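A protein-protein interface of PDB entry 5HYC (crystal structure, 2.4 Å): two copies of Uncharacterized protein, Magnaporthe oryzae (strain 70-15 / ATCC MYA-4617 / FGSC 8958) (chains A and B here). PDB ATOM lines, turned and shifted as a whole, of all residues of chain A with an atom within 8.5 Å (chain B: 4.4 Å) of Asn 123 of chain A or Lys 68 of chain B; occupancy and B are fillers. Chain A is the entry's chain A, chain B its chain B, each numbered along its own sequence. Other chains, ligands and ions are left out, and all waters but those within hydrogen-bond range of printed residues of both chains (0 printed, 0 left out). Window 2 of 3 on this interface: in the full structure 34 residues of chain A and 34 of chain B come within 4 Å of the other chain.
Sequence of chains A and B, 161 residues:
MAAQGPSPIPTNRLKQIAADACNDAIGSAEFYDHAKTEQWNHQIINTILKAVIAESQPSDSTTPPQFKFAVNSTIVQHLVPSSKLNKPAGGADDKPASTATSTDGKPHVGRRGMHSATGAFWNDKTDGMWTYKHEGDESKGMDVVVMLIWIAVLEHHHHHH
The backbone NH (N) of Phe 121 of chain A sits at hydrogen-bond distance from the backbone carbonyl oxygen (O) of Phe 69 of chain B.
The side-chain carboxylate of Asp 127 of chain A lies within salt-bridge range of the side-chain amino group of Lys 68 of chain B (2.5 Å).
The backbone carbonyl oxygen (O) of Asp 127 of chain A is in hydrogen-bond range of the backbone NH (N) of Gly 5 of chain A, 3.0 Å away.
OD1 of Asn 123 of chain A lies close to N of Lys 125 of chain A, 3.3 Å away.
The backbone NH (N) of Asn 123 of chain A lies within hydrogen-bond range of the side-chain carboxylate (OD2) of Asp 127 of chain A (3.1 Å).
OG1 of Thr 126 of chain A lies within hydrogen-bond range of OD1 of Asp 127 of chain A.
OD1 of Asp 127 of chain A sits at hydrogen-bond distance from N of Ala 152 of chain A.
The backbone carbonyl oxygen of Ile 151 of chain B lies within hydrogen-bond range of the backbone NH of Lys 68 of chain B (2.6 Å).
Lys 68 of chain A touches Ile 151 of chain B.
CA of Ala 120 of chain A touches O of Phe 69 of chain B, at 3.3 Å.
CD2 of Phe 121 of chain A touches O of Phe 67 of chain B, 3.8 Å away.
CA of Lys 68 of chain B touches O of Phe 121 of chain A, 3.4 Å away.
Phe 69 of chain B touches Trp 122 of chain A (O to CD1, 3.9 Å).
CB of Asn 123 of chain A touches NZ of Lys 68 of chain B, 3.8 Å away.
Ile 151 of chain A touches Lys 68 of chain B (CG2 to NZ, 3.5 Å).
Lys 68 of chain B touches Ala 152 of chain A (NZ to O, 3.9 Å).
Asn 123 of chain A touches one residue of chain B.
Lys 68 of chain B touches five residues of chain A.
Of the printed residues of chain B, Phe 121 of chain A touches Phe 67 (3.8 Å), Lys 68 (3.4 Å) and Phe 69 (2.7 Å).
Printed residues of chain B within 4 Å of Ala 120 of chain A: Phe 69.
Printed residues of chain A within 4 Å of Phe 67 of chain B: Phe 121 (3.8 Å).
Of the printed residues of chain A, Phe 69 of chain B touches Ala 120, Phe 121 and Trp 122.
Phe 67 of chain A touches none of the printed residues of chain B.
The nearest printed residue of chain A that does not touch Lys 68 of chain B is Thr 126 of chain A (4.3 Å).
The nearest printed residue of chain B that does not touch Ile 151 of chain A is Ile 151 of chain B (4.2 Å).
Hydrophobic or aromatic side chains of chain B that line the printed part of chain A: Ile 151.
Of the 18 printed residues of chain A, 8 touch a printed residue of chain B.
Printed residues of chain A that touch a printed residue of chain B: Lys 68, Ala 120, Phe 121, Trp 122, Asn 123, Asp 127, Ile 151 and Ala 152.
Along chain A the printed residues that touch a printed residue of chain B span positions 68 to 152.
Among the printed residues, 10 pairs touch across the chains.
Lys 68 of chain A touches Ile 151 of chain B, and with the chains exchanged Ile 151 of chain A touches Lys 68 of chain B.
5 positions are printed for both chains.
Of the 10 pairs that touch across the chains among the printed residues, 2 have their exchanged pair printed and touching as well.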
ATOM      1  N   GLY A   5      -3.133 -27.581  -6.821  1.00  0.00           N
ATOM      2  CA  GLY A   5      -3.747 -28.582  -7.673  1.00  0.00           C
ATOM      3  C   GLY A   5      -5.039 -28.101  -8.302  1.00  0.00           C
ATOM      4  O   GLY A   5      -5.185 -26.915  -8.590  1.00  0.00           O
ATOM      5  N   GLN A  66     -14.708 -23.711   2.967  1.00  0.00           N
ATOM      6  CA  GLN A  66     -13.568 -24.586   2.727  1.00  0.00           C
ATOM      7  C   GLN A  66     -12.349 -23.885   2.110  1.00  0.00           C
ATOM      8  O   GLN A  66     -11.243 -24.402   2.181  1.00  0.00           O
ATOM      9  CB  GLN A  66     -14.006 -25.749   1.842  1.00  0.00           C
ATOM     10  CG  GLN A  66     -15.055 -26.619   2.507  1.00  0.00           C
ATOM     11  CD  GLN A  66     -15.470 -27.795   1.663  1.00  0.00           C
ATOM     12  OE1 GLN A  66     -15.971 -27.633   0.554  1.00  0.00           O
ATOM     13  NE2 GLN A  66     -15.262 -28.996   2.185  1.00  0.00           N
ATOM     14  N   PHE A  67     -12.547 -22.706   1.533  1.00  0.00           N
ATOM     15  CA  PHE A  67     -11.441 -21.984   0.896  1.00  0.00           C
ATOM     16  C   PHE A  67     -11.337 -20.532   1.288  1.00  0.00           C
ATOM     17  O   PHE A  67     -12.330 -19.869   1.517  1.00  0.00           O
ATOM     18  CB  PHE A  67     -11.559 -22.050  -0.627  1.00  0.00           C
ATOM     19  CG  PHE A  67     -11.306 -23.404  -1.188  1.00  0.00           C
ATOM     20  CD1 PHE A  67     -10.018 -23.831  -1.436  1.00  0.00           C
ATOM     21  CD2 PHE A  67     -12.360 -24.262  -1.452  1.00  0.00           C
ATOM     22  CE1 PHE A  67      -9.783 -25.091  -1.944  1.00  0.00           C
ATOM     23  CE2 PHE A  67     -12.132 -25.526  -1.963  1.00  0.00           C
ATOM     24  CZ  PHE A  67     -10.845 -25.943  -2.210  1.00  0.00           C
ATOM     25  N   LYS A  68     -10.109 -20.040   1.335  1.00  0.00           N
ATOM     26  CA  LYS A  68      -9.863 -18.609   1.266  1.00  0.00           C
ATOM     27  C   LYS A  68      -9.627 -18.214  -0.203  1.00  0.00           C
ATOM     28  O   LYS A  68      -9.136 -19.019  -0.989  1.00  0.00           O
ATOM     29  CB  LYS A  68      -8.686 -18.234   2.163  1.00  0.00           C
ATOM     30  CG  LYS A  68      -9.038 -18.369   3.636  1.00  0.00           C
ATOM     31  CD  LYS A  68      -7.821 -18.408   4.546  1.00  0.00           C
ATOM     32  CE  LYS A  68      -8.243 -18.403   6.028  1.00  0.00           C
ATOM     33  NZ  LYS A  68      -7.078 -18.376   6.953  1.00  0.00           N
ATOM     34  N   GLY A 119       4.847 -16.641  -7.462  1.00  0.00           N
ATOM     35  CA  GLY A 119       5.358 -17.765  -6.701  1.00  0.00           C
ATOM     36  C   GLY A 119       4.626 -17.915  -5.376  1.00  0.00           C
ATOM     37  O   GLY A 119       4.010 -16.969  -4.885  1.00  0.00           O
ATOM     38  N   ALA A 120       4.694 -19.103  -4.788  1.00  0.00           N
ATOM     39  CA  ALA A 120       3.941 -19.375  -3.571  1.00  0.00           C
ATOM     40  C   ALA A 120       4.640 -20.337  -2.616  1.00  0.00           C
ATOM     41  O   ALA A 120       5.397 -21.198  -3.026  1.00  0.00           O
ATOM     42  CB  ALA A 120       2.558 -19.917  -3.931  1.00  0.00           C
ATOM     43  N   PHE A 121       4.385 -20.155  -1.326  1.00  0.00           N
ATOM     44  CA  PHE A 121       4.789 -21.109  -0.298  1.00  0.00           C
ATOM     45  C   PHE A 121       3.495 -21.645   0.293  1.00  0.00           C
ATOM     46  O   PHE A 121       2.870 -21.011   1.140  1.00  0.00           O
ATOM     47  CB  PHE A 121       5.680 -20.457   0.753  1.00  0.00           C
ATOM     48  CG  PHE A 121       6.172 -21.409   1.808  1.00  0.00           C
ATOM     49  CD1 PHE A 121       7.004 -22.463   1.472  1.00  0.00           C
ATOM     50  CD2 PHE A 121       5.813 -21.241   3.134  1.00  0.00           C
ATOM     51  CE1 PHE A 121       7.463 -23.336   2.429  1.00  0.00           C
ATOM     52  CE2 PHE A 121       6.263 -22.113   4.097  1.00  0.00           C
ATOM     53  CZ  PHE A 121       7.092 -23.166   3.746  1.00  0.00           C
ATOM     54  N   TRP A 122       3.116 -22.827  -0.183  1.00  0.00           N
ATOM     55  CA  TRP A 122       1.730 -23.285  -0.216  1.00  0.00           C
ATOM     56  C   TRP A 122       1.607 -24.736   0.115  1.00  0.00           C
ATOM     57  O   TRP A 122       2.589 -25.443   0.128  1.00  0.00           O
ATOM     58  CB  TRP A 122       1.155 -23.143  -1.621  1.00  0.00           C
ATOM     59  CG  TRP A 122       0.404 -21.957  -1.917  1.00  0.00           C
ATOM     60  CD1 TRP A 122       0.128 -20.924  -1.086  1.00  0.00           C
ATOM     61  CD2 TRP A 122      -0.209 -21.653  -3.165  1.00  0.00           C
ATOM     62  NE1 TRP A 122      -0.618 -19.973  -1.748  1.00  0.00           N
ATOM     63  CE2 TRP A 122      -0.840 -20.404  -3.027  1.00  0.00           C
ATOM     64  CE3 TRP A 122      -0.277 -22.311  -4.390  1.00  0.00           C
ATOM     65  CZ2 TRP A 122      -1.535 -19.806  -4.067  1.00  0.00           C
ATOM     66  CZ3 TRP A 122      -0.963 -21.715  -5.416  1.00  0.00           C
ATOM     67  CH2 TRP A 122      -1.587 -20.479  -5.250  1.00  0.00           C
ATOM     68  N   ASN A 123       0.372 -25.189   0.276  1.00  0.00           N
ATOM     69  CA  ASN A 123       0.059 -26.598   0.144  1.00  0.00           C
ATOM     70  C   ASN A 123      -0.176 -26.875  -1.340  1.00  0.00           C
ATOM     71  O   ASN A 123      -1.154 -26.420  -1.920  1.00  0.00           O
ATOM     72  CB  ASN A 123      -1.162 -26.974   0.983  1.00  0.00           C
ATOM     73  CG  ASN A 123      -1.311 -28.476   1.171  1.00  0.00           C
ATOM     74  OD1 ASN A 123      -1.057 -29.265   0.263  1.00  0.00           O
ATOM     75  ND2 ASN A 123      -1.736 -28.874   2.361  1.00  0.00           N
ATOM     76  N   ASP A 124       0.745 -27.613  -1.948  1.00  0.00           N
ATOM     77  CA  ASP A 124       0.763 -27.844  -3.391  1.00  0.00           C
ATOM     78  C   ASP A 124      -0.457 -28.624  -3.888  1.00  0.00           C
ATOM     79  O   ASP A 124      -0.887 -28.457  -5.027  1.00  0.00           O
ATOM     80  CB  ASP A 124       2.052 -28.580  -3.765  1.00  0.00           C
ATOM     81  CG  ASP A 124       2.164 -28.864  -5.256  1.00  0.00           C
ATOM     82  OD1 ASP A 124       1.690 -28.033  -6.056  1.00  0.00           O
ATOM     83  OD2 ASP A 124       2.748 -29.911  -5.625  1.00  0.00           O
ATOM     84  N   LYS A 125      -1.029 -29.456  -3.028  1.00  0.00           N
ATOM     85  CA  LYS A 125      -2.142 -30.305  -3.442  1.00  0.00           C
ATOM     86  C   LYS A 125      -3.526 -29.679  -3.252  1.00  0.00           C
ATOM     87  O   LYS A 125      -4.501 -30.153  -3.826  1.00  0.00           O
ATOM     88  CB  LYS A 125      -2.074 -31.644  -2.700  1.00  0.00           C
ATOM     89  CG  LYS A 125      -0.893 -32.506  -3.118  1.00  0.00           C
ATOM     90  CD  LYS A 125      -0.149 -33.091  -1.941  1.00  0.00           C
ATOM     91  CE  LYS A 125       0.840 -34.173  -2.390  1.00  0.00           C
ATOM     92  NZ  LYS A 125       1.506 -33.882  -3.694  1.00  0.00           N
ATOM     93  N   THR A 126      -3.611 -28.608  -2.472  1.00  0.00           N
ATOM     94  CA  THR A 126      -4.903 -27.993  -2.199  1.00  0.00           C
ATOM     95  C   THR A 126      -5.025 -26.571  -2.733  1.00  0.00           C
ATOM     96  O   THR A 126      -6.113 -26.122  -3.067  1.00  0.00           O
ATOM     97  CB  THR A 126      -5.197 -27.966  -0.695  1.00  0.00           C
ATOM     98  OG1 THR A 126      -4.184 -27.209  -0.025  1.00  0.00           O
ATOM     99  CG2 THR A 126      -5.213 -29.358  -0.147  1.00  0.00           C
ATOM    100  N   ASP A 127      -3.902 -25.875  -2.811  1.00  0.00           N
ATOM    101  CA  ASP A 127      -3.905 -24.460  -3.145  1.00  0.00           C
ATOM    102  C   ASP A 127      -3.510 -24.220  -4.594  1.00  0.00           C
ATOM    103  O   ASP A 127      -2.803 -25.027  -5.200  1.00  0.00           O
ATOM    104  CB  ASP A 127      -2.988 -23.712  -2.178  1.00  0.00           C
ATOM    105  CG  ASP A 127      -3.314 -24.031  -0.725  1.00  0.00           C
ATOM    106  OD1 ASP A 127      -4.476 -24.385  -0.460  1.00  0.00           O
ATOM    107  OD2 ASP A 127      -2.431 -23.933   0.146  1.00  0.00           O
ATOM    108  N   GLY A 128      -3.987 -23.121  -5.161  1.00  0.00           N
ATOM    109  CA  GLY A 128      -3.838 -22.911  -6.586  1.00  0.00           C
ATOM    110  C   GLY A 128      -4.198 -21.540  -7.113  1.00  0.00           C
ATOM    111  O   GLY A 128      -4.673 -20.677  -6.391  1.00  0.00           O
ATOM    112  N   TRP A 150      -6.915 -19.602  -4.688  1.00  0.00           N
ATOM    113  CA  TRP A 150      -7.672 -20.292  -3.660  1.00  0.00           C
ATOM    114  C   TRP A 150      -6.728 -20.956  -2.671  1.00  0.00           C
ATOM    115  O   TRP A 150      -5.781 -21.642  -3.050  1.00  0.00           O
ATOM    116  CB  TRP A 150      -8.626 -21.336  -4.259  1.00  0.00           C
ATOM    117  CG  TRP A 150      -7.958 -22.402  -5.080  1.00  0.00           C
ATOM    118  CD1 TRP A 150      -7.452 -23.591  -4.632  1.00  0.00           C
ATOM    119  CD2 TRP A 150      -7.751 -22.388  -6.498  1.00  0.00           C
ATOM    120  NE1 TRP A 150      -6.926 -24.309  -5.682  1.00  0.00           N
ATOM    121  CE2 TRP A 150      -7.096 -23.592  -6.838  1.00  0.00           C
ATOM    122  CE3 TRP A 150      -8.045 -21.471  -7.512  1.00  0.00           C
ATOM    123  CZ2 TRP A 150      -6.729 -23.894  -8.146  1.00  0.00           C
ATOM    124  CZ3 TRP A 150      -7.685 -21.778  -8.801  1.00  0.00           C
ATOM    125  CH2 TRP A 150      -7.031 -22.975  -9.108  1.00  0.00           C
ATOM    126  N   ILE A 151      -6.988 -20.725  -1.395  1.00  0.00           N
ATOM    127  CA  ILE A 151      -6.249 -21.385  -0.348  1.00  0.00           C
ATOM    128  C   ILE A 151      -7.225 -22.245   0.435  1.00  0.00           C
ATOM    129  O   ILE A 151      -8.197 -21.742   0.992  1.00  0.00           O
ATOM    130  CB  ILE A 151      -5.569 -20.391   0.591  1.00  0.00           C
ATOM    131  CG1 ILE A 151      -4.909 -19.252  -0.193  1.00  0.00           C
ATOM    132  CG2 ILE A 151      -4.579 -21.110   1.487  1.00  0.00           C
ATOM    133  CD1 ILE A 151      -3.418 -19.410  -0.376  1.00  0.00           C
ATOM    134  N   ALA A 152      -6.978 -23.549   0.464  1.00  0.00           N
ATOM    135  CA  ALA A 152      -7.856 -24.456   1.185  1.00  0.00           C
ATOM    136  C   ALA A 152      -7.854 -24.160   2.677  1.00  0.00           C
ATOM    137  O   ALA A 152      -6.824 -23.803   3.245  1.00  0.00           O
ATOM    138  CB  ALA A 152      -7.459 -25.879   0.943  1.00  0.00           C
ATOM    139  N   VAL A 153      -9.030 -24.272   3.285  1.00  0.00           N
ATOM    140  CA  VAL A 153      -9.146 -24.334   4.736  1.00  0.00           C
ATOM    141  C   VAL A 153      -8.732 -23.040   5.421  1.00  0.00           C
ATOM    142  O   VAL A 153      -9.415 -22.575   6.334  1.00  0.00           O
ATOM    143  CB  VAL A 153      -8.310 -25.505   5.286  1.00  0.00           C
ATOM    144  CG1 VAL A 153      -7.786 -25.204   6.673  1.00  0.00           C
ATOM    145  CG2 VAL A 153      -9.124 -26.778   5.254  1.00  0.00           C
ATOM    146  N   PHE B  67       2.675 -19.665   8.317  1.00  0.00           N
ATOM    147  CA  PHE B  67       2.048 -18.874   7.260  1.00  0.00           C
ATOM    148  C   PHE B  67       2.134 -19.526   5.895  1.00  0.00           C
ATOM    149  O   PHE B  67       3.099 -20.209   5.575  1.00  0.00           O
ATOM    150  CB  PHE B  67       2.678 -17.492   7.166  1.00  0.00           C
ATOM    151  CG  PHE B  67       2.309 -16.575   8.283  1.00  0.00           C
ATOM    152  CD1 PHE B  67       1.102 -15.895   8.268  1.00  0.00           C
ATOM    153  CD2 PHE B  67       3.174 -16.377   9.346  1.00  0.00           C
ATOM    154  CE1 PHE B  67       0.762 -15.040   9.293  1.00  0.00           C
ATOM    155  CE2 PHE B  67       2.837 -15.522  10.373  1.00  0.00           C
ATOM    156  CZ  PHE B  67       1.628 -14.855  10.346  1.00  0.00           C
ATOM    157  N   LYS B  68       1.101 -19.314   5.096  1.00  0.00           N
ATOM    158  CA  LYS B  68       1.217 -19.521   3.670  1.00  0.00           C
ATOM    159  C   LYS B  68       1.502 -18.165   3.034  1.00  0.00           C
ATOM    160  O   LYS B  68       0.954 -17.152   3.455  1.00  0.00           O
ATOM    161  CB  LYS B  68      -0.042 -20.154   3.103  1.00  0.00           C
ATOM    162  CG  LYS B  68      -0.149 -21.639   3.400  1.00  0.00           C
ATOM    163  CD  LYS B  68      -1.530 -22.125   3.058  1.00  0.00           C
ATOM    164  CE  LYS B  68      -1.657 -23.620   3.168  1.00  0.00           C
ATOM    165  NZ  LYS B  68      -2.951 -24.057   2.563  1.00  0.00           N
ATOM    166  N   PHE B  69       2.392 -18.146   2.046  1.00  0.00           N
ATOM    167  CA  PHE B  69       2.739 -16.906   1.360  1.00  0.00           C
ATOM    168  C   PHE B  69       2.540 -17.025  -0.143  1.00  0.00           C
ATOM    169  O   PHE B  69       2.766 -18.079  -0.723  1.00  0.00           O
ATOM    170  CB  PHE B  69       4.187 -16.517   1.635  1.00  0.00           C
ATOM    171  CG  PHE B  69       4.497 -16.250   3.078  1.00  0.00           C
ATOM    172  CD1 PHE B  69       4.013 -15.116   3.707  1.00  0.00           C
ATOM    173  CD2 PHE B  69       5.320 -17.102   3.785  1.00  0.00           C
ATOM    174  CE1 PHE B  69       4.317 -14.855   5.021  1.00  0.00           C
ATOM    175  CE2 PHE B  69       5.632 -16.851   5.113  1.00  0.00           C
ATOM    176  CZ  PHE B  69       5.135 -15.722   5.728  1.00  0.00           C
ATOM    177  N   ILE B 149       0.939 -11.757  -0.337  1.00  0.00           N
ATOM    178  CA  ILE B 149      -0.199 -12.230   0.426  1.00  0.00           C
ATOM    179  C   ILE B 149       0.248 -13.230   1.486  1.00  0.00           C
ATOM    180  O   ILE B 149       1.013 -14.142   1.181  1.00  0.00           O
ATOM    181  CB  ILE B 149      -1.254 -12.864  -0.496  1.00  0.00           C
ATOM    182  CG1 ILE B 149      -1.951 -11.764  -1.290  1.00  0.00           C
ATOM    183  CG2 ILE B 149      -2.276 -13.643   0.308  1.00  0.00           C
ATOM    184  CD1 ILE B 149      -2.984 -12.258  -2.261  1.00  0.00           C
ATOM    185  N   TRP B 150      -0.206 -13.049   2.728  1.00  0.00           N
ATOM    186  CA  TRP B 150       0.060 -14.034   3.779  1.00  0.00           C
ATOM    187  C   TRP B 150      -1.215 -14.602   4.378  1.00  0.00           C
ATOM    188  O   TRP B 150      -2.160 -13.873   4.670  1.00  0.00           O
ATOM    189  CB  TRP B 150       0.927 -13.445   4.907  1.00  0.00           C
ATOM    190  CG  TRP B 150       0.297 -12.332   5.667  1.00  0.00           C
ATOM    191  CD1 TRP B 150      -0.475 -12.438   6.784  1.00  0.00           C
ATOM    192  CD2 TRP B 150       0.399 -10.932   5.381  1.00  0.00           C
ATOM    193  NE1 TRP B 150      -0.872 -11.195   7.206  1.00  0.00           N
ATOM    194  CE2 TRP B 150      -0.350 -10.252   6.361  1.00  0.00           C
ATOM    195  CE3 TRP B 150       1.040 -10.188   4.384  1.00  0.00           C
ATOM    196  CZ2 TRP B 150      -0.471  -8.867   6.377  1.00  0.00           C
ATOM    197  CZ3 TRP B 150       0.924  -8.814   4.405  1.00  0.00           C
ATOM    198  CH2 TRP B 150       0.173  -8.166   5.389  1.00  0.00           C
ATOM    199  N   ILE B 151      -1.227 -15.918   4.547  1.00  0.00           N
ATOM    200  CA  ILE B 151      -2.357 -16.622   5.129  1.00  0.00           C
ATOM    201  C   ILE B 151      -1.874 -17.467   6.312  1.00  0.00           C
ATOM    202  O   ILE B 151      -1.071 -18.385   6.146  1.00  0.00           O
ATOM    203  CB  ILE B 151      -3.067 -17.528   4.088  1.00  0.00           C
ATOM    204  CG1 ILE B 151      -3.618 -16.706   2.912  1.00  0.00           C
ATOM    205  CG2 ILE B 151      -4.184 -18.320   4.733  1.00  0.00           C
ATOM    206  CD1 ILE B 151      -4.732 -15.756   3.272  1.00  0.00           C
ATOM    207  N   VAL B 153      -1.514 -20.165   9.139  1.00  0.00           N
ATOM    208  CA  VAL B 153      -1.822 -21.569   9.389  1.00  0.00           C
ATOM    209  C   VAL B 153      -2.551 -22.244   8.235  1.00  0.00           C
ATOM    210  O   VAL B 153      -2.346 -21.889   7.076  1.00  0.00           O
ATOM    211  CB  VAL B 153      -2.657 -21.712  10.665  1.00  0.00           C
ATOM    212  CG1 VAL B 153      -3.285 -23.087  10.737  1.00  0.00           C
ATOM    213  CG2 VAL B 153      -1.784 -21.438  11.874  1.00  0.00           C
